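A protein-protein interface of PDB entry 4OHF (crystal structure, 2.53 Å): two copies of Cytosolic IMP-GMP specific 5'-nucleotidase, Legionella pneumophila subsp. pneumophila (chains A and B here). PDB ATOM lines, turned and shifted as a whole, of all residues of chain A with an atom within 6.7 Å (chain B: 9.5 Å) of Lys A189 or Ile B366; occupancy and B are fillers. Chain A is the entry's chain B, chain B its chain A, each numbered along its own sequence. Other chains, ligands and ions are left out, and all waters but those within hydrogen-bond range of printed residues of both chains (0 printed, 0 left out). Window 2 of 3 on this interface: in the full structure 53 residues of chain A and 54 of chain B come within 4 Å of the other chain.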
ATOM      1  N   HIS A   4      11.410 -20.603 -14.762  1.00  0.00           N
ATOM      2  CA  HIS A   4      10.822 -20.920 -13.458  1.00  0.00           C
ATOM      3  C   HIS A   4       9.307 -20.670 -13.428  1.00  0.00           C
ATOM      4  O   HIS A   4       8.786 -20.059 -12.499  1.00  0.00           O
ATOM      5  CB  HIS A   4      11.492 -20.091 -12.352  1.00  0.00           C
ATOM      6  CG  HIS A   4      12.844 -20.592 -11.932  1.00  0.00           C
ATOM      7  ND1 HIS A   4      13.041 -21.843 -11.381  1.00  0.00           N
ATOM      8  CD2 HIS A   4      14.058 -19.987 -11.932  1.00  0.00           C
ATOM      9  CE1 HIS A   4      14.315 -21.987 -11.059  1.00  0.00           C
ATOM     10  NE2 HIS A   4      14.954 -20.877 -11.383  1.00  0.00           N
ATOM     11  N   ARG A 187      22.117 -31.908  -7.237  1.00  0.00           N
ATOM     12  CA  ARG A 187      22.208 -30.805  -6.289  1.00  0.00           C
ATOM     13  C   ARG A 187      21.839 -29.506  -6.993  1.00  0.00           C
ATOM     14  O   ARG A 187      22.079 -29.341  -8.187  1.00  0.00           O
ATOM     15  CB  ARG A 187      23.622 -30.717  -5.734  1.00  0.00           C
ATOM     16  CG  ARG A 187      23.963 -31.832  -4.755  1.00  0.00           C
ATOM     17  CD  ARG A 187      25.465 -32.050  -4.676  1.00  0.00           C
ATOM     18  NE  ARG A 187      25.896 -32.389  -3.323  1.00  0.00           N
ATOM     19  CZ  ARG A 187      27.142 -32.715  -2.999  1.00  0.00           C
ATOM     20  NH1 ARG A 187      28.083 -32.750  -3.938  1.00  0.00           N
ATOM     21  NH2 ARG A 187      27.445 -32.990  -1.736  1.00  0.00           N
ATOM     22  N   GLU A 188      21.245 -28.579  -6.260  1.00  0.00           N
ATOM     23  CA  GLU A 188      20.828 -27.321  -6.858  1.00  0.00           C
ATOM     24  C   GLU A 188      20.839 -26.210  -5.826  1.00  0.00           C
ATOM     25  O   GLU A 188      20.020 -26.203  -4.910  1.00  0.00           O
ATOM     26  CB  GLU A 188      19.418 -27.469  -7.459  1.00  0.00           C
ATOM     27  CG  GLU A 188      18.777 -26.162  -7.943  1.00  0.00           C
ATOM     28  CD  GLU A 188      17.347 -26.343  -8.457  1.00  0.00           C
ATOM     29  OE1 GLU A 188      16.711 -25.327  -8.815  1.00  0.00           O
ATOM     30  OE2 GLU A 188      16.860 -27.493  -8.508  1.00  0.00           O
ATOM     31  N   LYS A 189      21.770 -25.276  -5.979  1.00  0.00           N
ATOM     32  CA  LYS A 189      21.878 -24.145  -5.066  1.00  0.00           C
ATOM     33  C   LYS A 189      20.549 -23.415  -4.885  1.00  0.00           C
ATOM     34  O   LYS A 189      20.155 -23.091  -3.770  1.00  0.00           O
ATOM     35  CB  LYS A 189      22.937 -23.156  -5.574  1.00  0.00           C
ATOM     36  CG  LYS A 189      23.028 -21.868  -4.757  1.00  0.00           C
ATOM     37  CD  LYS A 189      24.292 -21.043  -5.045  1.00  0.00           C
ATOM     38  CE  LYS A 189      24.351 -20.516  -6.484  1.00  0.00           C
ATOM     39  NZ  LYS A 189      24.510 -21.597  -7.503  1.00  0.00           N
ATOM     40  N   GLU A 190      19.855 -23.170  -5.983  1.00  0.00           N
ATOM     41  CA  GLU A 190      18.586 -22.462  -5.929  1.00  0.00           C
ATOM     42  C   GLU A 190      17.611 -22.973  -4.857  1.00  0.00           C
ATOM     43  O   GLU A 190      16.940 -22.179  -4.198  1.00  0.00           O
ATOM     44  CB  GLU A 190      17.912 -22.497  -7.304  1.00  0.00           C
ATOM     45  CG  GLU A 190      18.646 -21.736  -8.426  1.00  0.00           C
ATOM     46  CD  GLU A 190      20.054 -22.280  -8.740  1.00  0.00           C
ATOM     47  OE1 GLU A 190      20.227 -23.506  -8.933  1.00  0.00           O
ATOM     48  OE2 GLU A 190      21.000 -21.464  -8.809  1.00  0.00           O
ATOM     49  N   VAL A 191      17.526 -24.290  -4.680  1.00  0.00           N
ATOM     50  CA  VAL A 191      16.613 -24.856  -3.691  1.00  0.00           C
ATOM     51  C   VAL A 191      16.881 -24.265  -2.318  1.00  0.00           C
ATOM     52  O   VAL A 191      15.962 -23.798  -1.654  1.00  0.00           O
ATOM     53  CB  VAL A 191      16.734 -26.406  -3.596  1.00  0.00           C
ATOM     54  CG1 VAL A 191      15.964 -26.915  -2.392  1.00  0.00           C
ATOM     55  CG2 VAL A 191      16.195 -27.051  -4.853  1.00  0.00           C
ATOM     56  N   VAL A 192      18.145 -24.290  -1.899  1.00  0.00           N
ATOM     57  CA  VAL A 192      18.524 -23.750  -0.601  1.00  0.00           C
ATOM     58  C   VAL A 192      18.237 -22.254  -0.516  1.00  0.00           C
ATOM     59  O   VAL A 192      17.658 -21.782   0.466  1.00  0.00           O
ATOM     60  CB  VAL A 192      20.014 -24.029  -0.298  1.00  0.00           C
ATOM     61  CG1 VAL A 192      20.491 -23.188   0.871  1.00  0.00           C
ATOM     62  CG2 VAL A 192      20.187 -25.503   0.049  1.00  0.00           C
ATOM     63  N   GLU A 193      18.629 -21.507  -1.538  1.00  0.00           N
ATOM     64  CA  GLU A 193      18.361 -20.074  -1.526  1.00  0.00           C
ATOM     65  C   GLU A 193      16.856 -19.860  -1.415  1.00  0.00           C
ATOM     66  O   GLU A 193      16.389 -18.996  -0.664  1.00  0.00           O
ATOM     67  CB  GLU A 193      18.879 -19.398  -2.800  1.00  0.00           C
ATOM     68  CG  GLU A 193      20.383 -19.504  -3.033  1.00  0.00           C
ATOM     69  CD  GLU A 193      21.211 -19.362  -1.744  1.00  0.00           C
ATOM     70  OE1 GLU A 193      20.928 -18.435  -0.936  1.00  0.00           O
ATOM     71  OE2 GLU A 193      22.152 -20.179  -1.545  1.00  0.00           O
ATOM     72  N   GLY A 194      16.104 -20.664  -2.161  1.00  0.00           N
ATOM     73  CA  GLY A 194      14.657 -20.568  -2.159  1.00  0.00           C
ATOM     74  C   GLY A 194      14.034 -20.776  -0.799  1.00  0.00           C
ATOM     75  O   GLY A 194      13.166 -20.010  -0.380  1.00  0.00           O
ATOM     76  N   ALA A 223      22.670 -33.138  -0.060  1.00  0.00           N
ATOM     77  CA  ALA A 223      22.109 -32.212  -1.041  1.00  0.00           C
ATOM     78  C   ALA A 223      21.850 -30.759  -0.640  1.00  0.00           C
ATOM     79  O   ALA A 223      21.635 -29.917  -1.509  1.00  0.00           O
ATOM     80  CB  ALA A 223      20.835 -32.812  -1.628  1.00  0.00           C
ATOM     81  N   PHE A 227      25.410 -25.719   0.286  1.00  0.00           N
ATOM     82  CA  PHE A 227      25.020 -24.336  -0.011  1.00  0.00           C
ATOM     83  C   PHE A 227      24.629 -23.520   1.214  1.00  0.00           C
ATOM     84  O   PHE A 227      23.973 -22.481   1.098  1.00  0.00           O
ATOM     85  CB  PHE A 227      23.847 -24.329  -0.994  1.00  0.00           C
ATOM     86  CG  PHE A 227      24.008 -25.286  -2.125  1.00  0.00           C
ATOM     87  CD1 PHE A 227      24.920 -25.036  -3.139  1.00  0.00           C
ATOM     88  CD2 PHE A 227      23.253 -26.457  -2.165  1.00  0.00           C
ATOM     89  CE1 PHE A 227      25.082 -25.936  -4.184  1.00  0.00           C
ATOM     90  CE2 PHE A 227      23.407 -27.364  -3.206  1.00  0.00           C
ATOM     91  CZ  PHE A 227      24.326 -27.102  -4.218  1.00  0.00           C
ATOM     92  N   GLU A 439      11.211 -19.567  -6.246  1.00  0.00           N
ATOM     93  CA  GLU A 439      11.809 -18.404  -6.887  1.00  0.00           C
ATOM     94  C   GLU A 439      10.765 -17.283  -6.992  1.00  0.00           C
ATOM     95  O   GLU A 439      11.067 -16.156  -7.366  1.00  0.00           O
ATOM     96  CB  GLU A 439      12.290 -18.788  -8.285  1.00  0.00           C
ATOM     97  CG  GLU A 439      13.586 -18.141  -8.681  1.00  0.00           C
ATOM     98  CD  GLU A 439      14.765 -18.770  -7.971  1.00  0.00           C
ATOM     99  OE1 GLU A 439      15.235 -19.836  -8.429  1.00  0.00           O
ATOM    100  OE2 GLU A 439      15.211 -18.206  -6.948  1.00  0.00           O
ATOM    101  N   TYR B 358       9.781 -10.156 -12.102  1.00  0.00           N
ATOM    102  CA  TYR B 358      10.087 -10.359 -10.681  1.00  0.00           C
ATOM    103  C   TYR B 358      11.016 -11.555 -10.465  1.00  0.00           C
ATOM    104  O   TYR B 358      12.091 -11.415  -9.896  1.00  0.00           O
ATOM    105  CB  TYR B 358       8.808 -10.587  -9.862  1.00  0.00           C
ATOM    106  CG  TYR B 358       9.066 -10.819  -8.380  1.00  0.00           C
ATOM    107  CD1 TYR B 358       8.985  -9.768  -7.460  1.00  0.00           C
ATOM    108  CD2 TYR B 358       9.398 -12.086  -7.895  1.00  0.00           C
ATOM    109  CE1 TYR B 358       9.223  -9.976  -6.097  1.00  0.00           C
ATOM    110  CE2 TYR B 358       9.641 -12.303  -6.530  1.00  0.00           C
ATOM    111  CZ  TYR B 358       9.549 -11.244  -5.639  1.00  0.00           C
ATOM    112  OH  TYR B 358       9.773 -11.448  -4.291  1.00  0.00           O
ATOM    113  N   VAL B 359      10.577 -12.732 -10.908  1.00  0.00           N
ATOM    114  CA  VAL B 359      11.364 -13.943 -10.757  1.00  0.00           C
ATOM    115  C   VAL B 359      12.715 -13.810 -11.447  1.00  0.00           C
ATOM    116  O   VAL B 359      13.709 -14.328 -10.951  1.00  0.00           O
ATOM    117  CB  VAL B 359      10.613 -15.197 -11.293  1.00  0.00           C
ATOM    118  CG1 VAL B 359       9.317 -15.389 -10.520  1.00  0.00           C
ATOM    119  CG2 VAL B 359      10.321 -15.056 -12.767  1.00  0.00           C
ATOM    120  N   ASP B 360      12.768 -13.111 -12.578  1.00  0.00           N
ATOM    121  CA  ASP B 360      14.042 -12.928 -13.266  1.00  0.00           C
ATOM    122  C   ASP B 360      15.033 -12.241 -12.328  1.00  0.00           C
ATOM    123  O   ASP B 360      16.145 -12.726 -12.142  1.00  0.00           O
ATOM    124  CB  ASP B 360      13.860 -12.116 -14.552  1.00  0.00           C
ATOM    125  CG  ASP B 360      13.118 -12.897 -15.629  1.00  0.00           C
ATOM    126  OD1 ASP B 360      12.839 -12.332 -16.714  1.00  0.00           O
ATOM    127  OD2 ASP B 360      12.809 -14.085 -15.383  1.00  0.00           O
ATOM    128  N   LEU B 361      14.636 -11.128 -11.720  1.00  0.00           N
ATOM    129  CA  LEU B 361      15.520 -10.429 -10.790  1.00  0.00           C
ATOM    130  C   LEU B 361      15.814 -11.292  -9.570  1.00  0.00           C
ATOM    131  O   LEU B 361      16.952 -11.391  -9.138  1.00  0.00           O
ATOM    132  CB  LEU B 361      14.898  -9.100 -10.356  1.00  0.00           C
ATOM    133  CG  LEU B 361      14.988  -7.970 -11.389  1.00  0.00           C
ATOM    134  CD1 LEU B 361      14.429  -8.428 -12.728  1.00  0.00           C
ATOM    135  CD2 LEU B 361      14.232  -6.755 -10.885  1.00  0.00           C
ATOM    136  N   CYS B 362      14.780 -11.920  -9.023  1.00  0.00           N
ATOM    137  CA  CYS B 362      14.924 -12.796  -7.857  1.00  0.00           C
ATOM    138  C   CYS B 362      15.855 -13.968  -8.186  1.00  0.00           C
ATOM    139  O   CYS B 362      16.565 -14.483  -7.318  1.00  0.00           O
ATOM    140  CB  CYS B 362      13.543 -13.331  -7.431  1.00  0.00           C
ATOM    141  SG  CYS B 362      13.534 -14.569  -6.075  1.00  0.00           S
ATOM    142  N   THR B 363      15.837 -14.383  -9.449  1.00  0.00           N
ATOM    143  CA  THR B 363      16.664 -15.485  -9.930  1.00  0.00           C
ATOM    144  C   THR B 363      18.017 -14.925 -10.375  1.00  0.00           C
ATOM    145  O   THR B 363      18.975 -15.669 -10.573  1.00  0.00           O
ATOM    146  CB  THR B 363      15.978 -16.207 -11.131  1.00  0.00           C
ATOM    147  OG1 THR B 363      16.347 -17.590 -11.141  1.00  0.00           O
ATOM    148  CG2 THR B 363      16.393 -15.578 -12.455  1.00  0.00           C
ATOM    149  N   ARG B 364      18.078 -13.604 -10.521  1.00  0.00           N
ATOM    150  CA  ARG B 364      19.288 -12.903 -10.947  1.00  0.00           C
ATOM    151  C   ARG B 364      20.130 -12.506  -9.742  1.00  0.00           C
ATOM    152  O   ARG B 364      21.264 -12.059  -9.883  1.00  0.00           O
ATOM    153  CB  ARG B 364      18.899 -11.655 -11.740  1.00  0.00           C
ATOM    154  CG  ARG B 364      20.049 -10.829 -12.283  1.00  0.00           C
ATOM    155  CD  ARG B 364      19.502  -9.694 -13.132  1.00  0.00           C
ATOM    156  NE  ARG B 364      20.551  -8.965 -13.837  1.00  0.00           N
ATOM    157  CZ  ARG B 364      21.482  -8.227 -13.239  1.00  0.00           C
ATOM    158  NH1 ARG B 364      22.400  -7.599 -13.968  1.00  0.00           N
ATOM    159  NH2 ARG B 364      21.491  -8.113 -11.916  1.00  0.00           N
ATOM    160  N   SER B 365      19.561 -12.662  -8.552  1.00  0.00           N
ATOM    161  CA  SER B 365      20.261 -12.328  -7.322  1.00  0.00           C
ATOM    162  C   SER B 365      20.940 -13.570  -6.758  1.00  0.00           C
ATOM    163  O   SER B 365      21.549 -13.526  -5.692  1.00  0.00           O
ATOM    164  CB  SER B 365      19.279 -11.755  -6.300  1.00  0.00           C
ATOM    165  OG  SER B 365      18.741 -10.520  -6.745  1.00  0.00           O
ATOM    166  N   ILE B 366      20.818 -14.680  -7.477  1.00  0.00           N
ATOM    167  CA  ILE B 366      21.432 -15.942  -7.067  1.00  0.00           C
ATOM    168  C   ILE B 366      22.608 -16.240  -8.009  1.00  0.00           C
ATOM    169  O   ILE B 366      23.558 -16.942  -7.637  1.00  0.00           O
ATOM    170  CB  ILE B 366      20.416 -17.112  -7.121  1.00  0.00           C
ATOM    171  CG1 ILE B 366      19.147 -16.735  -6.348  1.00  0.00           C
ATOM    172  CG2 ILE B 366      21.040 -18.379  -6.521  1.00  0.00           C
ATOM    173  CD1 ILE B 366      18.051 -17.776  -6.420  1.00  0.00           C
ATOM    174  N   ASP B 367      22.524 -15.701  -9.227  1.00  0.00           N
ATOM    175  CA  ASP B 367      23.573 -15.858 -10.234  1.00  0.00           C
ATOM    176  C   ASP B 367      24.624 -14.765 -10.022  1.00  0.00           C
ATOM    177  O   ASP B 367      25.443 -14.492 -10.905  1.00  0.00           O
ATOM    178  CB  ASP B 367      23.008 -15.733 -11.660  1.00  0.00           C
ATOM    179  CG  ASP B 367      22.138 -16.918 -12.064  1.00  0.00           C
ATOM    180  OD1 ASP B 367      22.491 -18.074 -11.746  1.00  0.00           O
ATOM    181  OD2 ASP B 367      21.105 -16.687 -12.728  1.00  0.00           O
ATOM    182  N   GLU B 368      24.581 -14.138  -8.848  1.00  0.00           N
ATOM    183  CA  GLU B 368      25.521 -13.083  -8.486  1.00  0.00           C
ATOM    184  C   GLU B 368      25.180 -12.523  -7.110  1.00  0.00           C
ATOM    185  O   GLU B 368      25.379 -11.334  -6.846  1.00  0.00           O
ATOM    186  CB  GLU B 368      25.497 -11.962  -9.531  1.00  0.00           C
ATOM    187  CG  GLU B 368      24.132 -11.355  -9.783  1.00  0.00           C
ATOM    188  CD  GLU B 368      24.183 -10.201 -10.773  1.00  0.00           C
ATOM    189  OE1 GLU B 368      24.727  -9.131 -10.424  1.00  0.00           O
ATOM    190  OE2 GLU B 368      23.682 -10.365 -11.905  1.00  0.00           O
ATOM    191  N   SER B 369      24.670 -13.397  -6.246  1.00  0.00           N
ATOM    192  CA  SER B 369      24.277 -13.050  -4.878  1.00  0.00           C
ATOM    193  C   SER B 369      24.019 -11.557  -4.673  1.00  0.00           C
ATOM    194  O   SER B 369      24.916 -10.805  -4.290  1.00  0.00           O
ATOM    195  CB  SER B 369      25.340 -13.528  -3.884  1.00  0.00           C
ATOM    196  OG  SER B 369      25.505 -14.936  -3.944  1.00  0.00           O
ATOM    197  N   ILE B 377      13.109  -4.799  -6.566  1.00  0.00           N
ATOM    198  CA  ILE B 377      12.154  -5.884  -6.443  1.00  0.00           C
ATOM    199  C   ILE B 377      10.906  -5.373  -5.718  1.00  0.00           C
ATOM    200  O   ILE B 377       9.776  -5.629  -6.140  1.00  0.00           O
ATOM    201  CB  ILE B 377      12.792  -7.036  -5.656  1.00  0.00           C
ATOM    202  CG1 ILE B 377      13.810  -7.742  -6.551  1.00  0.00           C
ATOM    203  CG2 ILE B 377      11.730  -7.972  -5.118  1.00  0.00           C
ATOM    204  CD1 ILE B 377      14.601  -8.815  -5.852  1.00  0.00           C
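NE2 of His A4 lies within hydrogen-bond range of OE1 of Glu A439, 3.1 Å away.
NZ of Lys A189 is in salt-bridge range of OE2 of Glu A190 (3.7 Å).
No position is printed for both chains.
Of the 8 pairs that touch across the chains among the printed residues, none has its exchanged pair printed and touching as well.
Among the printed residues, pairs that only touch across the chains: His A4 with Thr B363 (3.4 Å), Lys A189 with Ile B366 (3.8 Å), Glu A190 with Ile B366 (3.8 Å), Glu A193 with Ile B366 (3.7 Å), Glu A439 with Val B359 (3.7 Å), Glu A439 with Thr B363 (3.7 Å) and Glu A439 with Ile B366 (2.9 Å).
SG of Cys B362 lies within hydrogen-bond range of O of Glu A439, at 3.2 Å.
No residue of chain B comes within 4 Å of Val A192.
Phe A227 touches none of the printed residues of chain B.
Of the printed residues of chain B, Glu A439 touches Val B359 (3.7 Å), Cys B362 (3.2 Å), Thr B363 (3.7 Å) and Ile B366 (2.9 Å).
Of the printed residues of chain A, Val B359 touches Glu A439 (3.7 Å).
Arg B364 touches none of the printed residues of chain A.
Ile B366 touches four residues of chain A.
The nearest residue of chain B that does not touch Lys A189 is Asp B367 (5.8 Å).
The nearest residue of chain A that does not touch Ile B366 is Gly A194 (5.5 Å).
The nearest printed residue of chain B that does not touch Glu A439 is Tyr B358 (4.2 Å).
Hydrophobic or aromatic side chains of chain B within 4 Å of the printed part of chain A: Val B359 and Ile B366.
Among the printed residues, no Asp or Glu carboxylate lies within 4 Å of a Lys or Arg side-chain nitrogen of the other chain.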
